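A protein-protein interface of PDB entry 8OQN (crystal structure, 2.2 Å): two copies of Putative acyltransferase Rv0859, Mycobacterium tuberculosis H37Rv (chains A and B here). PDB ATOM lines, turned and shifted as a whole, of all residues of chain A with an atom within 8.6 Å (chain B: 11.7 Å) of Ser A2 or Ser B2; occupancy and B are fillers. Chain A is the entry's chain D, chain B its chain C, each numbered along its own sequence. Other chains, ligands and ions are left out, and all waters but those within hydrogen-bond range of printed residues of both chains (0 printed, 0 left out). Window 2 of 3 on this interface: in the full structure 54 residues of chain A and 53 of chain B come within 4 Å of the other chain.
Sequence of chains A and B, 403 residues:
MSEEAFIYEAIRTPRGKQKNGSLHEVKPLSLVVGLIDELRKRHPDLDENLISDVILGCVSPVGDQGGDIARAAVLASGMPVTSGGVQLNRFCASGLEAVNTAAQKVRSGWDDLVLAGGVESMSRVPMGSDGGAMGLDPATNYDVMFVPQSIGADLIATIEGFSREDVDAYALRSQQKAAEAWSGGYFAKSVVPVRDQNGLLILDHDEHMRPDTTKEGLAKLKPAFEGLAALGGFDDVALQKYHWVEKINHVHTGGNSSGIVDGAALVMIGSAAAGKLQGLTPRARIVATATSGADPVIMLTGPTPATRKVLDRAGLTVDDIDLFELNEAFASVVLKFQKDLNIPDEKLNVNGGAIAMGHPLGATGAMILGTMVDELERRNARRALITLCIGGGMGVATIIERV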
ATOM      1  N   SER A   2     -17.419 -30.254  -3.886  1.00  0.00           N
ATOM      2  CA  SER A   2     -18.497 -31.066  -4.437  1.00  0.00           C
ATOM      3  C   SER A   2     -18.611 -32.391  -3.693  1.00  0.00           C
ATOM      4  O   SER A   2     -19.490 -32.565  -2.849  1.00  0.00           O
ATOM      5  CB  SER A   2     -18.273 -31.315  -5.928  1.00  0.00           C
ATOM      6  OG  SER A   2     -19.357 -32.029  -6.495  1.00  0.00           O
ATOM      7  N   GLU A   3     -17.722 -33.327  -4.014  1.00  0.00           N
ATOM      8  CA  GLU A   3     -17.685 -34.596  -3.305  1.00  0.00           C
ATOM      9  C   GLU A   3     -17.205 -34.392  -1.873  1.00  0.00           C
ATOM     10  O   GLU A   3     -16.406 -33.499  -1.583  1.00  0.00           O
ATOM     11  CB  GLU A   3     -16.772 -35.589  -4.023  1.00  0.00           C
ATOM     12  CG  GLU A   3     -17.480 -36.447  -5.053  1.00  0.00           C
ATOM     13  CD  GLU A   3     -17.279 -37.931  -4.803  1.00  0.00           C
ATOM     14  OE1 GLU A   3     -16.273 -38.487  -5.291  1.00  0.00           O
ATOM     15  OE2 GLU A   3     -18.121 -38.536  -4.106  1.00  0.00           O
ATOM     16  N   GLU A   4     -17.707 -35.229  -0.968  1.00  0.00           N
ATOM     17  CA  GLU A   4     -17.321 -35.158   0.433  1.00  0.00           C
ATOM     18  C   GLU A   4     -16.094 -36.022   0.689  1.00  0.00           C
ATOM     19  O   GLU A   4     -15.951 -37.105   0.114  1.00  0.00           O
ATOM     20  CB  GLU A   4     -18.471 -35.602   1.337  1.00  0.00           C
ATOM     21  CG  GLU A   4     -19.641 -34.635   1.357  1.00  0.00           C
ATOM     22  CD  GLU A   4     -19.285 -33.303   1.989  1.00  0.00           C
ATOM     23  OE1 GLU A   4     -18.436 -33.286   2.905  1.00  0.00           O
ATOM     24  OE2 GLU A   4     -19.853 -32.272   1.567  1.00  0.00           O
ATOM     25  N   ALA A   5     -15.210 -35.535   1.556  1.00  0.00           N
ATOM     26  CA  ALA A   5     -13.957 -36.207   1.880  1.00  0.00           C
ATOM     27  C   ALA A   5     -14.037 -36.785   3.287  1.00  0.00           C
ATOM     28  O   ALA A   5     -14.324 -36.061   4.246  1.00  0.00           O
ATOM     29  CB  ALA A   5     -12.776 -35.240   1.771  1.00  0.00           C
ATOM     30  N   ALA A 103      -7.779 -33.964   1.115  1.00  0.00           N
ATOM     31  CA  ALA A 103      -9.225 -33.761   1.133  1.00  0.00           C
ATOM     32  C   ALA A 103      -9.680 -32.916  -0.049  1.00  0.00           C
ATOM     33  O   ALA A 103     -10.706 -33.213  -0.673  1.00  0.00           O
ATOM     34  CB  ALA A 103      -9.647 -33.106   2.446  1.00  0.00           C
ATOM     35  N   GLN A 104      -8.935 -31.856  -0.370  1.00  0.00           N
ATOM     36  CA  GLN A 104      -9.321 -30.996  -1.483  1.00  0.00           C
ATOM     37  C   GLN A 104      -9.157 -31.704  -2.822  1.00  0.00           C
ATOM     38  O   GLN A 104      -9.921 -31.440  -3.758  1.00  0.00           O
ATOM     39  CB  GLN A 104      -8.512 -29.699  -1.442  1.00  0.00           C
ATOM     40  CG  GLN A 104      -8.829 -28.840  -0.224  1.00  0.00           C
ATOM     41  CD  GLN A 104      -7.922 -27.631  -0.091  1.00  0.00           C
ATOM     42  OE1 GLN A 104      -6.723 -27.762   0.154  1.00  0.00           O
ATOM     43  NE2 GLN A 104      -8.496 -26.441  -0.243  1.00  0.00           N
ATOM     44  N   VAL A 106      -9.789 -34.883  -3.162  1.00  0.00           N
ATOM     45  CA  VAL A 106     -10.982 -35.721  -3.216  1.00  0.00           C
ATOM     46  C   VAL A 106     -12.208 -34.889  -3.567  1.00  0.00           C
ATOM     47  O   VAL A 106     -13.059 -35.312  -4.358  1.00  0.00           O
ATOM     48  CB  VAL A 106     -11.165 -36.467  -1.882  1.00  0.00           C
ATOM     49  CG1 VAL A 106     -12.534 -37.128  -1.819  1.00  0.00           C
ATOM     50  CG2 VAL A 106     -10.066 -37.500  -1.705  1.00  0.00           C
ATOM     51  N   ARG A 107     -12.313 -33.686  -2.994  1.00  0.00           N
ATOM     52  CA  ARG A 107     -13.488 -32.853  -3.224  1.00  0.00           C
ATOM     53  C   ARG A 107     -13.568 -32.363  -4.663  1.00  0.00           C
ATOM     54  O   ARG A 107     -14.670 -32.144  -5.179  1.00  0.00           O
ATOM     55  CB  ARG A 107     -13.490 -31.665  -2.265  1.00  0.00           C
ATOM     56  CG  ARG A 107     -13.825 -32.029  -0.832  1.00  0.00           C
ATOM     57  CD  ARG A 107     -13.855 -30.802   0.052  1.00  0.00           C
ATOM     58  NE  ARG A 107     -14.777 -29.776  -0.424  1.00  0.00           N
ATOM     59  CZ  ARG A 107     -16.040 -29.657  -0.032  1.00  0.00           C
ATOM     60  NH1 ARG A 107     -16.583 -30.512   0.820  1.00  0.00           N
ATOM     61  NH2 ARG A 107     -16.775 -28.656  -0.508  1.00  0.00           N
ATOM     62  N   SER A 108     -12.424 -32.184  -5.327  1.00  0.00           N
ATOM     63  CA  SER A 108     -12.433 -31.745  -6.718  1.00  0.00           C
ATOM     64  C   SER A 108     -12.939 -32.820  -7.670  1.00  0.00           C
ATOM     65  O   SER A 108     -13.159 -32.523  -8.849  1.00  0.00           O
ATOM     66  CB  SER A 108     -11.031 -31.304  -7.144  1.00  0.00           C
ATOM     67  OG  SER A 108     -10.180 -32.420  -7.343  1.00  0.00           O
ATOM     68  N   GLY A 109     -13.129 -34.049  -7.195  1.00  0.00           N
ATOM     69  CA  GLY A 109     -13.591 -35.131  -8.037  1.00  0.00           C
ATOM     70  C   GLY A 109     -12.525 -35.777  -8.890  1.00  0.00           C
ATOM     71  O   GLY A 109     -12.825 -36.752  -9.593  1.00  0.00           O
ATOM     72  N   TRP A 110     -11.289 -35.282  -8.846  1.00  0.00           N
ATOM     73  CA  TRP A 110     -10.218 -35.780  -9.695  1.00  0.00           C
ATOM     74  C   TRP A 110      -9.317 -36.795  -9.001  1.00  0.00           C
ATOM     75  O   TRP A 110      -8.435 -37.364  -9.653  1.00  0.00           O
ATOM     76  CB  TRP A 110      -9.387 -34.603 -10.217  1.00  0.00           C
ATOM     77  CG  TRP A 110     -10.169 -33.714 -11.151  1.00  0.00           C
ATOM     78  CD1 TRP A 110     -11.305 -34.043 -11.836  1.00  0.00           C
ATOM     79  CD2 TRP A 110      -9.881 -32.350 -11.489  1.00  0.00           C
ATOM     80  NE1 TRP A 110     -11.734 -32.974 -12.587  1.00  0.00           N
ATOM     81  CE2 TRP A 110     -10.878 -31.922 -12.389  1.00  0.00           C
ATOM     82  CE3 TRP A 110      -8.877 -31.450 -11.119  1.00  0.00           C
ATOM     83  CZ2 TRP A 110     -10.898 -30.636 -12.926  1.00  0.00           C
ATOM     84  CZ3 TRP A 110      -8.897 -30.173 -11.655  1.00  0.00           C
ATOM     85  CH2 TRP A 110      -9.899 -29.781 -12.552  1.00  0.00           C
ATOM     86  N   SER A 271     -13.330 -40.481  -0.938  1.00  0.00           N
ATOM     87  CA  SER A 271     -14.731 -40.149  -1.114  1.00  0.00           C
ATOM     88  C   SER A 271     -15.611 -41.261  -0.547  1.00  0.00           C
ATOM     89  O   SER A 271     -15.142 -42.351  -0.210  1.00  0.00           O
ATOM     90  CB  SER A 271     -15.045 -39.920  -2.592  1.00  0.00           C
ATOM     91  OG  SER A 271     -14.892 -41.115  -3.341  1.00  0.00           O
ATOM     92  N   ARG A 285     -15.729 -36.832   8.913  1.00  0.00           N
ATOM     93  CA  ARG A 285     -15.861 -36.047   7.695  1.00  0.00           C
ATOM     94  C   ARG A 285     -15.091 -34.745   7.855  1.00  0.00           C
ATOM     95  O   ARG A 285     -15.131 -34.118   8.918  1.00  0.00           O
ATOM     96  CB  ARG A 285     -17.331 -35.752   7.379  1.00  0.00           C
ATOM     97  CG  ARG A 285     -17.546 -34.962   6.096  1.00  0.00           C
ATOM     98  CD  ARG A 285     -19.026 -34.834   5.754  1.00  0.00           C
ATOM     99  NE  ARG A 285     -19.747 -33.999   6.708  1.00  0.00           N
ATOM    100  CZ  ARG A 285     -19.872 -32.682   6.605  1.00  0.00           C
ATOM    101  NH1 ARG A 285     -19.319 -32.011   5.608  1.00  0.00           N
ATOM    102  NH2 ARG A 285     -20.574 -32.023   7.522  1.00  0.00           N
ATOM    103  N   SER B   2     -17.637 -28.553  -8.262  1.00  0.00           N
ATOM    104  CA  SER B   2     -18.557 -27.427  -8.154  1.00  0.00           C
ATOM    105  C   SER B   2     -17.968 -26.186  -8.814  1.00  0.00           C
ATOM    106  O   SER B   2     -18.288 -25.869  -9.961  1.00  0.00           O
ATOM    107  CB  SER B   2     -18.891 -27.140  -6.688  1.00  0.00           C
ATOM    108  OG  SER B   2     -19.866 -26.117  -6.582  1.00  0.00           O
ATOM    109  N   GLU B   3     -17.108 -25.483  -8.082  1.00  0.00           N
ATOM    110  CA  GLU B   3     -16.427 -24.322  -8.637  1.00  0.00           C
ATOM    111  C   GLU B   3     -15.490 -24.748  -9.759  1.00  0.00           C
ATOM    112  O   GLU B   3     -14.806 -25.769  -9.663  1.00  0.00           O
ATOM    113  CB  GLU B   3     -15.634 -23.595  -7.551  1.00  0.00           C
ATOM    114  CG  GLU B   3     -16.468 -23.071  -6.392  1.00  0.00           C
ATOM    115  CD  GLU B   3     -17.205 -21.785  -6.725  1.00  0.00           C
ATOM    116  OE1 GLU B   3     -17.142 -21.336  -7.888  1.00  0.00           O
ATOM    117  OE2 GLU B   3     -17.845 -21.220  -5.812  1.00  0.00           O
ATOM    118  N   GLU B   4     -15.466 -23.961 -10.830  1.00  0.00           N
ATOM    119  CA  GLU B   4     -14.528 -24.181 -11.920  1.00  0.00           C
ATOM    120  C   GLU B   4     -13.269 -23.358 -11.685  1.00  0.00           C
ATOM    121  O   GLU B   4     -13.331 -22.237 -11.176  1.00  0.00           O
ATOM    122  CB  GLU B   4     -15.157 -23.816 -13.267  1.00  0.00           C
ATOM    123  CG  GLU B   4     -16.166 -24.835 -13.781  1.00  0.00           C
ATOM    124  CD  GLU B   4     -15.522 -26.151 -14.186  1.00  0.00           C
ATOM    125  OE1 GLU B   4     -14.325 -26.148 -14.547  1.00  0.00           O
ATOM    126  OE2 GLU B   4     -16.213 -27.190 -14.141  1.00  0.00           O
ATOM    127  N   ALA B   5     -12.124 -23.927 -12.049  1.00  0.00           N
ATOM    128  CA  ALA B   5     -10.837 -23.271 -11.876  1.00  0.00           C
ATOM    129  C   ALA B   5     -10.403 -22.642 -13.193  1.00  0.00           C
ATOM    130  O   ALA B   5     -10.350 -23.322 -14.223  1.00  0.00           O
ATOM    131  CB  ALA B   5      -9.781 -24.262 -11.385  1.00  0.00           C
ATOM    132  N   PHE B   6     -10.094 -21.349 -13.158  1.00  0.00           N
ATOM    133  CA  PHE B   6      -9.695 -20.606 -14.344  1.00  0.00           C
ATOM    134  C   PHE B   6      -8.262 -20.115 -14.204  1.00  0.00           C
ATOM    135  O   PHE B   6      -7.808 -19.775 -13.107  1.00  0.00           O
ATOM    136  CB  PHE B   6     -10.617 -19.403 -14.590  1.00  0.00           C
ATOM    137  CG  PHE B   6     -12.031 -19.780 -14.916  1.00  0.00           C
ATOM    138  CD1 PHE B   6     -12.408 -20.049 -16.223  1.00  0.00           C
ATOM    139  CD2 PHE B   6     -12.986 -19.865 -13.917  1.00  0.00           C
ATOM    140  CE1 PHE B   6     -13.712 -20.395 -16.525  1.00  0.00           C
ATOM    141  CE2 PHE B   6     -14.290 -20.209 -14.212  1.00  0.00           C
ATOM    142  CZ  PHE B   6     -14.654 -20.475 -15.518  1.00  0.00           C
ATOM    143  N   ALA B 103      -5.583 -25.663  -8.750  1.00  0.00           N
ATOM    144  CA  ALA B 103      -6.892 -25.832  -9.370  1.00  0.00           C
ATOM    145  C   ALA B 103      -7.822 -26.644  -8.478  1.00  0.00           C
ATOM    146  O   ALA B 103      -9.018 -26.345  -8.382  1.00  0.00           O
ATOM    147  CB  ALA B 103      -6.742 -26.496 -10.739  1.00  0.00           C
ATOM    148  N   GLN B 104      -7.287 -27.666  -7.804  1.00  0.00           N
ATOM    149  CA  GLN B 104      -8.118 -28.500  -6.942  1.00  0.00           C
ATOM    150  C   GLN B 104      -8.512 -27.776  -5.660  1.00  0.00           C
ATOM    151  O   GLN B 104      -9.603 -28.015  -5.126  1.00  0.00           O
ATOM    152  CB  GLN B 104      -7.394 -29.808  -6.629  1.00  0.00           C
ATOM    153  CG  GLN B 104      -7.276 -30.724  -7.838  1.00  0.00           C
ATOM    154  CD  GLN B 104      -6.308 -31.868  -7.622  1.00  0.00           C
ATOM    155  OE1 GLN B 104      -5.120 -31.656  -7.372  1.00  0.00           O
ATOM    156  NE2 GLN B 104      -6.811 -33.093  -7.722  1.00  0.00           N
ATOM    157  N   LYS B 105      -7.648 -26.894  -5.149  1.00  0.00           N
ATOM    158  CA  LYS B 105      -8.033 -26.061  -4.014  1.00  0.00           C
ATOM    159  C   LYS B 105      -9.185 -25.135  -4.380  1.00  0.00           C
ATOM    160  O   LYS B 105     -10.090 -24.903  -3.569  1.00  0.00           O
ATOM    161  CB  LYS B 105      -6.833 -25.250  -3.522  1.00  0.00           C
ATOM    162  CG  LYS B 105      -5.906 -25.999  -2.581  1.00  0.00           C
ATOM    163  CD  LYS B 105      -4.751 -25.112  -2.129  1.00  0.00           C
ATOM    164  CE  LYS B 105      -4.167 -25.586  -0.804  1.00  0.00           C
ATOM    165  NZ  LYS B 105      -3.663 -26.984  -0.873  1.00  0.00           N
ATOM    166  N   VAL B 106      -9.170 -24.595  -5.599  1.00  0.00           N
ATOM    167  CA  VAL B 106     -10.258 -23.730  -6.043  1.00  0.00           C
ATOM    168  C   VAL B 106     -11.541 -24.536  -6.215  1.00  0.00           C
ATOM    169  O   VAL B 106     -12.623 -24.108  -5.795  1.00  0.00           O
ATOM    170  CB  VAL B 106      -9.867 -23.006  -7.342  1.00  0.00           C
ATOM    171  CG1 VAL B 106     -11.076 -22.311  -7.947  1.00  0.00           C
ATOM    172  CG2 VAL B 106      -8.753 -22.006  -7.071  1.00  0.00           C
ATOM    173  N   ARG B 107     -11.438 -25.716  -6.834  1.00  0.00           N
ATOM    174  CA  ARG B 107     -12.621 -26.542  -7.052  1.00  0.00           C
ATOM    175  C   ARG B 107     -13.252 -26.988  -5.740  1.00  0.00           C
ATOM    176  O   ARG B 107     -14.474 -27.166  -5.668  1.00  0.00           O
ATOM    177  CB  ARG B 107     -12.268 -27.764  -7.898  1.00  0.00           C
ATOM    178  CG  ARG B 107     -12.250 -27.503  -9.389  1.00  0.00           C
ATOM    179  CD  ARG B 107     -11.978 -28.778 -10.162  1.00  0.00           C
ATOM    180  NE  ARG B 107     -13.075 -29.737 -10.102  1.00  0.00           N
ATOM    181  CZ  ARG B 107     -14.000 -29.877 -11.043  1.00  0.00           C
ATOM    182  NH1 ARG B 107     -14.008 -29.114 -12.123  1.00  0.00           N
ATOM    183  NH2 ARG B 107     -14.939 -30.808 -10.897  1.00  0.00           N
ATOM    184  N   SER B 108     -12.443 -27.174  -4.694  1.00  0.00           N
ATOM    185  CA  SER B 108     -12.973 -27.643  -3.419  1.00  0.00           C
ATOM    186  C   SER B 108     -13.834 -26.594  -2.728  1.00  0.00           C
ATOM    187  O   SER B 108     -14.599 -26.939  -1.821  1.00  0.00           O
ATOM    188  CB  SER B 108     -11.830 -28.066  -2.495  1.00  0.00           C
ATOM    189  OG  SER B 108     -11.226 -26.941  -1.882  1.00  0.00           O
ATOM    190  N   GLY B 109     -13.730 -25.329  -3.136  1.00  0.00           N
ATOM    191  CA  GLY B 109     -14.503 -24.259  -2.546  1.00  0.00           C
ATOM    192  C   GLY B 109     -13.862 -23.585  -1.352  1.00  0.00           C
ATOM    193  O   GLY B 109     -14.413 -22.597  -0.851  1.00  0.00           O
ATOM    194  N   TRP B 110     -12.716 -24.077  -0.887  1.00  0.00           N
ATOM    195  CA  TRP B 110     -12.063 -23.556   0.306  1.00  0.00           C
ATOM    196  C   TRP B 110     -10.939 -22.578  -0.006  1.00  0.00           C
ATOM    197  O   TRP B 110     -10.295 -22.076   0.920  1.00  0.00           O
ATOM    198  CB  TRP B 110     -11.535 -24.719   1.153  1.00  0.00           C
ATOM    199  CG  TRP B 110     -12.633 -25.602   1.667  1.00  0.00           C
ATOM    200  CD1 TRP B 110     -13.947 -25.266   1.824  1.00  0.00           C
ATOM    201  CD2 TRP B 110     -12.517 -26.969   2.077  1.00  0.00           C
ATOM    202  NE1 TRP B 110     -14.654 -26.336   2.313  1.00  0.00           N
ATOM    203  CE2 TRP B 110     -13.800 -27.394   2.477  1.00  0.00           C
ATOM    204  CE3 TRP B 110     -11.454 -27.875   2.149  1.00  0.00           C
ATOM    205  CZ2 TRP B 110     -14.047 -28.684   2.942  1.00  0.00           C
ATOM    206  CZ3 TRP B 110     -11.701 -29.154   2.610  1.00  0.00           C
ATOM    207  CH2 TRP B 110     -12.986 -29.545   3.007  1.00  0.00           C
ATOM    208  N   ASP B 111     -10.687 -22.301  -1.283  1.00  0.00           N
ATOM    209  CA  ASP B 111      -9.752 -21.270  -1.705  1.00  0.00           C
ATOM    210  C   ASP B 111     -10.341 -20.560  -2.914  1.00  0.00           C
ATOM    211  O   ASP B 111     -11.102 -21.148  -3.686  1.00  0.00           O
ATOM    212  CB  ASP B 111      -8.368 -21.848  -2.040  1.00  0.00           C
ATOM    213  CG  ASP B 111      -7.581 -22.241  -0.801  1.00  0.00           C
ATOM    214  OD1 ASP B 111      -7.138 -21.336  -0.061  1.00  0.00           O
ATOM    215  OD2 ASP B 111      -7.414 -23.457  -0.561  1.00  0.00           O
ATOM    216  N   ASP B 112      -9.993 -19.288  -3.066  1.00  0.00           N
ATOM    217  CA  ASP B 112     -10.575 -18.458  -4.113  1.00  0.00           C
ATOM    218  C   ASP B 112      -9.567 -17.995  -5.152  1.00  0.00           C
ATOM    219  O   ASP B 112      -9.894 -17.947  -6.340  1.00  0.00           O
ATOM    220  CB  ASP B 112     -11.255 -17.233  -3.489  1.00  0.00           C
ATOM    221  CG  ASP B 112     -12.185 -17.603  -2.348  1.00  0.00           C
ATOM    222  OD1 ASP B 112     -13.107 -18.419  -2.568  1.00  0.00           O
ATOM    223  OD2 ASP B 112     -11.984 -17.087  -1.227  1.00  0.00           O
ATOM    224  N   GLY B 270      -7.933 -19.066 -10.225  1.00  0.00           N
ATOM    225  CA  GLY B 270      -9.009 -18.651  -9.345  1.00  0.00           C
ATOM    226  C   GLY B 270     -10.362 -19.089  -9.855  1.00  0.00           C
ATOM    227  O   GLY B 270     -10.507 -19.595 -10.970  1.00  0.00           O
ATOM    228  N   SER B 271     -11.360 -18.885  -9.001  1.00  0.00           N
ATOM    229  CA  SER B 271     -12.742 -19.164  -9.345  1.00  0.00           C
ATOM    230  C   SER B 271     -13.306 -18.039 -10.209  1.00  0.00           C
ATOM    231  O   SER B 271     -12.677 -16.997 -10.413  1.00  0.00           O
ATOM    232  CB  SER B 271     -13.581 -19.340  -8.082  1.00  0.00           C
ATOM    233  OG  SER B 271     -13.694 -18.120  -7.370  1.00  0.00           O
ATOM    234  N   ALA B 272     -14.515 -18.265 -10.728  1.00  0.00           N
ATOM    235  CA  ALA B 272     -15.171 -17.236 -11.528  1.00  0.00           C
ATOM    236  C   ALA B 272     -15.511 -16.019 -10.679  1.00  0.00           C
ATOM    237  O   ALA B 272     -15.318 -14.876 -11.112  1.00  0.00           O
ATOM    238  CB  ALA B 272     -16.430 -17.800 -12.186  1.00  0.00           C
ATOM    239  N   ALA B 273     -16.013 -16.246  -9.462  1.00  0.00           N
ATOM    240  CA  ALA B 273     -16.366 -15.135  -8.585  1.00  0.00           C
ATOM    241  C   ALA B 273     -15.136 -14.323  -8.198  1.00  0.00           C
ATOM    242  O   ALA B 273     -15.202 -13.092  -8.105  1.00  0.00           O
ATOM    243  CB  ALA B 273     -17.079 -15.656  -7.338  1.00  0.00           C
ATOM    244  N   LYS B 276     -14.346 -12.206 -11.306  1.00  0.00           N
ATOM    245  CA  LYS B 276     -15.321 -11.126 -11.445  1.00  0.00           C
ATOM    246  C   LYS B 276     -15.083 -10.034 -10.411  1.00  0.00           C
ATOM    247  O   LYS B 276     -15.190  -8.841 -10.720  1.00  0.00           O
ATOM    248  CB  LYS B 276     -16.745 -11.668 -11.310  1.00  0.00           C
ATOM    249  CG  LYS B 276     -17.268 -12.444 -12.505  1.00  0.00           C
ATOM    250  CD  LYS B 276     -18.792 -12.465 -12.486  1.00  0.00           C
ATOM    251  CE  LYS B 276     -19.371 -13.390 -13.543  1.00  0.00           C
ATOM    252  NZ  LYS B 276     -19.416 -14.805 -13.079  1.00  0.00           N
ATOM    253  N   ARG B 285      -9.575 -22.540 -18.826  1.00  0.00           N
ATOM    254  CA  ARG B 285     -10.223 -23.297 -17.765  1.00  0.00           C
ATOM    255  C   ARG B 285      -9.543 -24.651 -17.630  1.00  0.00           C
ATOM    256  O   ARG B 285      -9.239 -25.303 -18.634  1.00  0.00           O
ATOM    257  CB  ARG B 285     -11.721 -23.487 -18.058  1.00  0.00           C
ATOM    258  CG  ARG B 285     -12.476 -24.304 -17.020  1.00  0.00           C
ATOM    259  CD  ARG B 285     -13.964 -24.398 -17.345  1.00  0.00           C
ATOM    260  NE  ARG B 285     -14.237 -25.268 -18.484  1.00  0.00           N
ATOM    261  CZ  ARG B 285     -14.475 -26.570 -18.388  1.00  0.00           C
ATOM    262  NH1 ARG B 285     -14.463 -27.191 -17.220  1.00  0.00           N
ATOM    263  NH2 ARG B 285     -14.733 -27.266 -19.492  1.00  0.00           N
ATOM    264  N   ILE B 286      -9.298 -25.067 -16.392  1.00  0.00           N
ATOM    265  CA  ILE B 286      -8.709 -26.376 -16.126  1.00  0.00           C
ATOM    266  C   ILE B 286      -9.818 -27.416 -16.245  1.00  0.00           C
ATOM    267  O   ILE B 286     -10.698 -27.502 -15.386  1.00  0.00           O
ATOM    268  CB  ILE B 286      -8.039 -26.430 -14.750  1.00  0.00           C
ATOM    269  CG1 ILE B 286      -7.079 -25.251 -14.567  1.00  0.00           C
ATOM    270  CG2 ILE B 286      -7.298 -27.744 -14.585  1.00  0.00           C
ATOM    271  CD1 ILE B 286      -5.791 -25.385 -15.336  1.00  0.00           C
ATOM    272  N   VAL B 287      -9.786 -28.201 -17.321  1.00  0.00           N
ATOM    273  CA  VAL B 287     -10.856 -29.159 -17.570  1.00  0.00           C
ATOM    274  C   VAL B 287     -10.727 -30.368 -16.654  1.00  0.00           C
ATOM    275  O   VAL B 287     -11.692 -30.769 -15.993  1.00  0.00           O
ATOM    276  CB  VAL B 287     -10.871 -29.572 -19.051  1.00  0.00           C
ATOM    277  CG1 VAL B 287     -11.891 -30.673 -19.277  1.00  0.00           C
ATOM    278  CG2 VAL B 287     -11.185 -28.373 -19.919  1.00  0.00           C
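The side-chain hydroxyl (OG) of Ser A108 lies close to the side-chain amide nitrogen (NE2) of Gln B104 (3.5 Å). The side-chain amide oxygen of Gln A104 is in hydrogen-bond range of the side-chain amino group of Lys B105 (3.3 Å). O of Ser A108 sits at hydrogen-bond distance from NE of Arg B107. NE2 of Gln A104 sits at hydrogen-bond distance from OG of Ser B108. The guanidinium group (NH2) of Arg A107 lies within hydrogen-bond range of the backbone carbonyl oxygen (O) of Ser B108 (3.1 Å). OD2 of Asp B111 sits at hydrogen-bond distance from NE2 of Gln A104, at 3.2 Å.
Ser A2 touches its own counterpart, Ser B2. Gln A104 touches its own counterpart, Gln B104. Gln A104 touches Trp B110, and with the chains exchanged Trp A110 touches Gln B104. Arg A107 touches Ser B108, and with the chains exchanged Ser A108 touches Arg B107.
Hydrophobic or aromatic side chains of chain B within 4 Å of the printed part of chain A: Trp B110 and Ile B286. Printed residues of chain A that touch a printed residue of chain B: Ser A2, Gln A104, Arg A107, Ser A108 and Trp A110. Along chain A the printed residues that touch a printed residue of chain B span positions 2 to 110. Among the printed residues, 14 pairs touch across the chains. Among the printed residues, no Asp or Glu carboxylate lies within 4 Å of a Lys or Arg side-chain nitrogen of the other chain.
The side-chain carboxylate (OE2) of Glu B4 is in salt-bridge range of the guanidinium group (NH1) of Arg B107 (3.6 Å). N of Ile B286 lies within hydrogen-bond range of O of Ala B5 (3.0 Å). O of Lys B105 sits at hydrogen-bond distance from OG of Ser B108, 2.9 Å away. The side-chain hydroxyl (OG) of Ser B108 lies close to the backbone NH (N) of Trp B110. NH1 of Arg A107 is in salt-bridge range of OE2 of Glu A4, at 3.8 Å. The side-chain hydroxyl (OG) of Ser A108 sits close to the backbone NH (N) of Trp A110, at 3.4 Å.
Printed residues of chain B within 4 Å of Ser A2: Ser B2. Of chain A, only Ser A2 comes within 4 Å of Ser B2. No residue of chain B comes within 4 Å of Glu A4. Arg A107 touches just these residues of chain B: Ser B108 and Trp B110. Of the printed residues of chain B, Ser A108 touches Gln B104 (3.4 Å) and Arg B107 (3.1 Å). Of the printed residues of chain A, Gln B104 touches Gln A104, Ser A108 and Trp A110. Printed residues of chain A within 4 Å of Asp B111: Gln A104. Of the printed residues of chain A, Lys B105 touches Gln A104. Arg B285 touches none of the printed residues of chain A. The nearest residue of chain B that does not touch Ser A2 is Arg B107 (4.6 Å). The nearest residue of chain A that does not touch Ser B2 is Arg A107 (5.6 Å). The nearest printed residue of chain A that does not touch Ser B108 is Ser A2 (4.8 Å).
Ser A2 touches Ser B2 (CB to N, 3.7 Å). O of Gln B104 touches O of Gln A104, 3.7 Å away. Gln A104 touches Trp B110. CD of Arg A107 touches CH2 of Trp B110, 3.3 Å away. Gln B104 touches Trp A110 (CG to CE3, 3.7 Å). Trp A110 touches Arg B107. Trp A110 touches Ile B286. Trp A110 touches Val B287 (CZ2 to O, 3.2 Å).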
